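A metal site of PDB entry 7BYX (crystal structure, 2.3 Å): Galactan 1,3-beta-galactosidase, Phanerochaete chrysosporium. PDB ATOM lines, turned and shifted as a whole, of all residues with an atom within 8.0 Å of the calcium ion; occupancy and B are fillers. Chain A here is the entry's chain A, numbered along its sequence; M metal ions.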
ATOM      1  N   TYR A 307      -4.172 -29.686 -21.651  1.00  0.00           N
ATOM      2  CA  TYR A 307      -2.888 -29.516 -20.992  1.00  0.00           C
ATOM      3  C   TYR A 307      -2.094 -28.494 -21.789  1.00  0.00           C
ATOM      4  O   TYR A 307      -1.729 -28.753 -22.934  1.00  0.00           O
ATOM      5  CB  TYR A 307      -2.115 -30.841 -20.917  1.00  0.00           C
ATOM      6  CG  TYR A 307      -2.831 -31.923 -20.166  1.00  0.00           C
ATOM      7  CD1 TYR A 307      -3.732 -32.742 -20.810  1.00  0.00           C
ATOM      8  CD2 TYR A 307      -2.595 -32.142 -18.808  1.00  0.00           C
ATOM      9  CE1 TYR A 307      -4.398 -33.760 -20.126  1.00  0.00           C
ATOM     10  CE2 TYR A 307      -3.243 -33.147 -18.120  1.00  0.00           C
ATOM     11  CZ  TYR A 307      -4.138 -33.952 -18.780  1.00  0.00           C
ATOM     12  OH  TYR A 307      -4.804 -34.945 -18.100  1.00  0.00           O
ATOM     13  N   GLU A 308      -1.824 -27.347 -21.180  1.00  0.00           N
ATOM     14  CA  GLU A 308      -1.002 -26.340 -21.833  1.00  0.00           C
ATOM     15  C   GLU A 308       0.442 -26.803 -21.944  1.00  0.00           C
ATOM     16  O   GLU A 308       1.008 -27.370 -21.006  1.00  0.00           O
ATOM     17  CB  GLU A 308      -1.070 -25.009 -21.069  1.00  0.00           C
ATOM     18  CG  GLU A 308      -2.484 -24.429 -20.981  1.00  0.00           C
ATOM     19  CD  GLU A 308      -3.027 -23.934 -22.332  1.00  0.00           C
ATOM     20  OE1 GLU A 308      -4.257 -23.858 -22.468  1.00  0.00           O
ATOM     21  OE2 GLU A 308      -2.233 -23.606 -23.249  1.00  0.00           O
ATOM     22  N   ALA A 309       1.046 -26.556 -23.106  1.00  0.00           N
ATOM     23  CA  ALA A 309       2.447 -26.937 -23.318  1.00  0.00           C
ATOM     24  C   ALA A 309       3.376 -26.158 -22.400  1.00  0.00           C
ATOM     25  O   ALA A 309       4.375 -26.700 -21.904  1.00  0.00           O
ATOM     26  CB  ALA A 309       2.813 -26.714 -24.788  1.00  0.00           C
ATOM     27  N   GLU A 310       3.044 -24.886 -22.131  1.00  0.00           N
ATOM     28  CA  GLU A 310       3.907 -24.029 -21.319  1.00  0.00           C
ATOM     29  C   GLU A 310       3.965 -24.460 -19.863  1.00  0.00           C
ATOM     30  O   GLU A 310       4.846 -24.000 -19.130  1.00  0.00           O
ATOM     31  CB  GLU A 310       3.426 -22.563 -21.389  1.00  0.00           C
ATOM     32  CG  GLU A 310       1.948 -22.366 -21.008  1.00  0.00           C
ATOM     33  CD  GLU A 310       1.025 -22.437 -22.222  1.00  0.00           C
ATOM     34  OE1 GLU A 310       1.366 -23.149 -23.203  1.00  0.00           O
ATOM     35  OE2 GLU A 310      -0.038 -21.780 -22.201  1.00  0.00           O
ATOM     36  N   ASN A 311       3.055 -25.326 -19.409  1.00  0.00           N
ATOM     37  CA  ASN A 311       3.152 -25.887 -18.066  1.00  0.00           C
ATOM     38  C   ASN A 311       3.947 -27.200 -18.022  1.00  0.00           C
ATOM     39  O   ASN A 311       4.161 -27.741 -16.936  1.00  0.00           O
ATOM     40  CB  ASN A 311       1.757 -26.136 -17.455  1.00  0.00           C
ATOM     41  CG  ASN A 311       0.965 -24.851 -17.289  1.00  0.00           C
ATOM     42  OD1 ASN A 311       1.524 -23.772 -17.070  1.00  0.00           O
ATOM     43  ND2 ASN A 311      -0.354 -24.958 -17.419  1.00  0.00           N
ATOM     44  N   ILE A 320       9.704 -20.557 -24.162  1.00  0.00           N
ATOM     45  CA  ILE A 320       8.340 -20.068 -24.229  1.00  0.00           C
ATOM     46  C   ILE A 320       8.202 -19.038 -25.350  1.00  0.00           C
ATOM     47  O   ILE A 320       9.101 -18.220 -25.598  1.00  0.00           O
ATOM     48  CB  ILE A 320       7.914 -19.478 -22.879  1.00  0.00           C
ATOM     49  CG1 ILE A 320       7.827 -20.599 -21.851  1.00  0.00           C
ATOM     50  CG2 ILE A 320       6.581 -18.740 -22.993  1.00  0.00           C
ATOM     51  CD1 ILE A 320       6.777 -21.617 -22.228  1.00  0.00           C
ATOM     52  N   LEU A 321       7.064 -19.086 -26.037  1.00  0.00           N
ATOM     53  CA  LEU A 321       6.642 -18.080 -27.008  1.00  0.00           C
ATOM     54  C   LEU A 321       5.319 -17.476 -26.549  1.00  0.00           C
ATOM     55  O   LEU A 321       4.526 -18.142 -25.868  1.00  0.00           O
ATOM     56  CB  LEU A 321       6.466 -18.700 -28.399  1.00  0.00           C
ATOM     57  CG  LEU A 321       7.698 -19.129 -29.176  1.00  0.00           C
ATOM     58  CD1 LEU A 321       7.242 -19.646 -30.518  1.00  0.00           C
ATOM     59  CD2 LEU A 321       8.600 -17.952 -29.383  1.00  0.00           C
ATOM     60  N   GLY A 323       1.765 -15.090 -27.807  1.00  0.00           N
ATOM     61  CA  GLY A 323       0.930 -14.677 -28.922  1.00  0.00           C
ATOM     62  C   GLY A 323      -0.534 -14.654 -28.548  1.00  0.00           C
ATOM     63  O   GLY A 323      -1.016 -15.526 -27.805  1.00  0.00           O
ATOM     64  N   GLY A 325      -2.799 -15.500 -30.457  1.00  0.00           N
ATOM     65  CA  GLY A 325      -3.375 -16.710 -31.037  1.00  0.00           C
ATOM     66  C   GLY A 325      -3.318 -17.938 -30.130  1.00  0.00           C
ATOM     67  O   GLY A 325      -3.955 -18.947 -30.455  1.00  0.00           O
ATOM     68  N   PHE A 326      -2.595 -17.879 -28.999  1.00  0.00           N
ATOM     69  CA  PHE A 326      -2.327 -19.053 -28.164  1.00  0.00           C
ATOM     70  C   PHE A 326      -3.286 -19.165 -26.982  1.00  0.00           C
ATOM     71  O   PHE A 326      -3.619 -18.164 -26.344  1.00  0.00           O
ATOM     72  CB  PHE A 326      -0.900 -19.039 -27.621  1.00  0.00           C
ATOM     73  CG  PHE A 326       0.155 -19.068 -28.675  1.00  0.00           C
ATOM     74  CD1 PHE A 326       0.050 -19.961 -29.736  1.00  0.00           C
ATOM     75  CD2 PHE A 326       1.247 -18.221 -28.607  1.00  0.00           C
ATOM     76  CE1 PHE A 326       1.038 -20.005 -30.714  1.00  0.00           C
ATOM     77  CE2 PHE A 326       2.241 -18.248 -29.587  1.00  0.00           C
ATOM     78  CZ  PHE A 326       2.136 -19.141 -30.648  1.00  0.00           C
ATOM     79  N   SER A 327      -3.652 -20.400 -26.663  1.00  0.00           N
ATOM     80  CA  SER A 327      -4.315 -20.664 -25.382  1.00  0.00           C
ATOM     81  C   SER A 327      -3.378 -20.297 -24.234  1.00  0.00           C
ATOM     82  O   SER A 327      -2.172 -20.554 -24.303  1.00  0.00           O
ATOM     83  CB  SER A 327      -4.719 -22.133 -25.324  1.00  0.00           C
ATOM     84  OG  SER A 327      -5.292 -22.459 -24.067  1.00  0.00           O
ATOM     85  N   GLY A 328      -3.916 -19.656 -23.214  1.00  0.00           N
ATOM     86  CA  GLY A 328      -3.088 -19.116 -22.140  1.00  0.00           C
ATOM     87  C   GLY A 328      -2.156 -17.986 -22.563  1.00  0.00           C
ATOM     88  O   GLY A 328      -1.380 -17.482 -21.747  1.00  0.00           O
ATOM     89  N   GLY A 329      -2.218 -17.589 -23.830  1.00  0.00           N
ATOM     90  CA  GLY A 329      -1.333 -16.564 -24.367  1.00  0.00           C
ATOM     91  C   GLY A 329       0.101 -16.995 -24.588  1.00  0.00           C
ATOM     92  O   GLY A 329       0.953 -16.143 -24.895  1.00  0.00           O
ATOM     93  N   LYS A 330       0.392 -18.294 -24.446  1.00  0.00           N
ATOM     94  CA  LYS A 330       1.762 -18.791 -24.506  1.00  0.00           C
ATOM     95  C   LYS A 330       1.815 -20.148 -25.188  1.00  0.00           C
ATOM     96  O   LYS A 330       0.850 -20.912 -25.172  1.00  0.00           O
ATOM     97  CB  LYS A 330       2.372 -18.918 -23.104  1.00  0.00           C
ATOM     98  CG  LYS A 330       2.716 -17.616 -22.433  1.00  0.00           C
ATOM     99  CD  LYS A 330       3.117 -17.858 -20.979  1.00  0.00           C
ATOM    100  CE  LYS A 330       2.091 -18.720 -20.271  1.00  0.00           C
ATOM    101  NZ  LYS A 330       2.374 -18.897 -18.799  1.00  0.00           N
ATOM    102  N   ALA A 331       2.984 -20.442 -25.750  1.00  0.00           N
ATOM    103  CA  ALA A 331       3.248 -21.723 -26.393  1.00  0.00           C
ATOM    104  C   ALA A 331       4.719 -22.064 -26.178  1.00  0.00           C
ATOM    105  O   ALA A 331       5.502 -21.223 -25.739  1.00  0.00           O
ATOM    106  CB  ALA A 331       2.922 -21.678 -27.897  1.00  0.00           C
ATOM    107  N   VAL A 332       5.090 -23.301 -26.496  1.00  0.00           N
ATOM    108  CA  VAL A 332       6.484 -23.732 -26.423  1.00  0.00           C
ATOM    109  C   VAL A 332       7.056 -23.739 -27.838  1.00  0.00           C
ATOM    110  O   VAL A 332       6.633 -24.541 -28.689  1.00  0.00           O
ATOM    111  CB  VAL A 332       6.628 -25.092 -25.739  1.00  0.00           C
ATOM    112  CG1 VAL A 332       8.067 -25.592 -25.816  1.00  0.00           C
ATOM    113  CG2 VAL A 332       6.173 -24.989 -24.306  1.00  0.00           C
ATOM    114  N   TYR A 358      -2.499 -28.916 -30.577  1.00  0.00           N
ATOM    115  CA  TYR A 358      -2.735 -27.532 -30.982  1.00  0.00           C
ATOM    116  C   TYR A 358      -1.379 -26.835 -31.199  1.00  0.00           C
ATOM    117  O   TYR A 358      -0.572 -26.774 -30.278  1.00  0.00           O
ATOM    118  CB  TYR A 358      -3.575 -26.794 -29.933  1.00  0.00           C
ATOM    119  CG  TYR A 358      -5.030 -27.162 -30.017  1.00  0.00           C
ATOM    120  CD1 TYR A 358      -5.465 -28.430 -29.669  1.00  0.00           C
ATOM    121  CD2 TYR A 358      -5.965 -26.258 -30.504  1.00  0.00           C
ATOM    122  CE1 TYR A 358      -6.775 -28.797 -29.767  1.00  0.00           C
ATOM    123  CE2 TYR A 358      -7.286 -26.608 -30.603  1.00  0.00           C
ATOM    124  CZ  TYR A 358      -7.680 -27.883 -30.242  1.00  0.00           C
ATOM    125  OH  TYR A 358      -8.986 -28.272 -30.344  1.00  0.00           O
ATOM    126  N   VAL A 392      -3.192 -20.831 -34.645  1.00  0.00           N
ATOM    127  CA  VAL A 392      -3.160 -22.199 -34.134  1.00  0.00           C
ATOM    128  C   VAL A 392      -4.264 -23.024 -34.782  1.00  0.00           C
ATOM    129  O   VAL A 392      -5.410 -22.572 -34.890  1.00  0.00           O
ATOM    130  CB  VAL A 392      -3.299 -22.209 -32.586  1.00  0.00           C
ATOM    131  CG1 VAL A 392      -3.585 -23.612 -32.056  1.00  0.00           C
ATOM    132  CG2 VAL A 392      -2.061 -21.595 -31.938  1.00  0.00           C
ATOM    133  N   LEU A 421       4.209 -25.575 -30.012  1.00  0.00           N
ATOM    134  CA  LEU A 421       3.139 -26.369 -29.424  1.00  0.00           C
ATOM    135  C   LEU A 421       2.380 -25.516 -28.400  1.00  0.00           C
ATOM    136  O   LEU A 421       2.977 -25.000 -27.449  1.00  0.00           O
ATOM    137  CB  LEU A 421       3.681 -27.641 -28.782  1.00  0.00           C
ATOM    138  CG  LEU A 421       2.638 -28.584 -28.170  1.00  0.00           C
ATOM    139  CD1 LEU A 421       1.695 -29.110 -29.270  1.00  0.00           C
ATOM    140  CD2 LEU A 421       3.301 -29.751 -27.440  1.00  0.00           C
ATOM    141  N   ASP A 422       1.080 -25.362 -28.606  1.00  0.00           N
ATOM    142  CA  ASP A 422       0.268 -24.479 -27.776  1.00  0.00           C
ATOM    143  C   ASP A 422      -0.280 -25.230 -26.567  1.00  0.00           C
ATOM    144  O   ASP A 422      -0.036 -24.830 -25.422  1.00  0.00           O
ATOM    145  CB  ASP A 422      -0.884 -23.903 -28.612  1.00  0.00           C
ATOM    146  CG  ASP A 422      -1.807 -22.978 -27.818  1.00  0.00           C
ATOM    147  OD1 ASP A 422      -1.523 -22.694 -26.639  1.00  0.00           O
ATOM    148  OD2 ASP A 422      -2.822 -22.514 -28.381  1.00  0.00           O
ATOM    149  N   LYS A 423      -1.007 -26.295 -26.824  1.00  0.00           N
ATOM    150  CA  LYS A 423      -1.576 -27.151 -25.801  1.00  0.00           C
ATOM    151  C   LYS A 423      -1.966 -28.450 -26.478  1.00  0.00           C
ATOM    152  O   LYS A 423      -1.856 -28.589 -27.707  1.00  0.00           O
ATOM    153  CB  LYS A 423      -2.773 -26.498 -25.104  1.00  0.00           C
ATOM    154  CG  LYS A 423      -3.986 -26.291 -26.027  1.00  0.00           C
ATOM    155  CD  LYS A 423      -5.264 -26.257 -25.220  1.00  0.00           C
ATOM    156  CE  LYS A 423      -6.475 -25.832 -26.042  1.00  0.00           C
ATOM    157  NZ  LYS A 423      -7.697 -25.985 -25.179  1.00  0.00           N
ATOM    158  N   ILE A 424      -2.423 -29.409 -25.676  1.00  0.00           N
ATOM    159  CA  ILE A 424      -2.972 -30.664 -26.152  1.00  0.00           C
ATOM    160  C   ILE A 424      -4.276 -30.909 -25.409  1.00  0.00           C
ATOM    161  O   ILE A 424      -4.505 -30.390 -24.309  1.00  0.00           O
ATOM    162  CB  ILE A 424      -2.013 -31.870 -25.935  1.00  0.00           C
ATOM    163  CG1 ILE A 424      -1.837 -32.180 -24.449  1.00  0.00           C
ATOM    164  CG2 ILE A 424      -0.650 -31.649 -26.606  1.00  0.00           C
ATOM    165  CD1 ILE A 424      -1.184 -33.509 -24.190  1.00  0.00           C
HETATM  166 CA    CA M   1      -0.725 -22.447 -24.464  1.00  0.00          CA
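The backbone carbonyl oxygen (O) of Asp 422 lies close to the backbone NH (N) of Ala 309, at 3.1 Å. N of Asp 422 lies within hydrogen-bond range of O of Tyr 358.
Of the 22 residues printed, 5 come within 4 Å of the calcium ion.
The calcium ion is bound by OE2 of Glu 308 (2.3 Å). The backbone carbonyl oxygen (O) of Lys 330 binds the calcium ion (2.3 Å). The calcium ion is bound by OD1 of Asp 422. The calcium ion is bound by O of Ser 327 (2.4 Å). The side-chain carboxylate (OE2) of Glu 310 binds the calcium ion, at 2.5 Å. OE1 of Glu 310 is bound to the calcium ion (2.5 Å). The calcium ion is bound by O of Asp 422. The calcium ion has seven donor atoms within binding distance.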
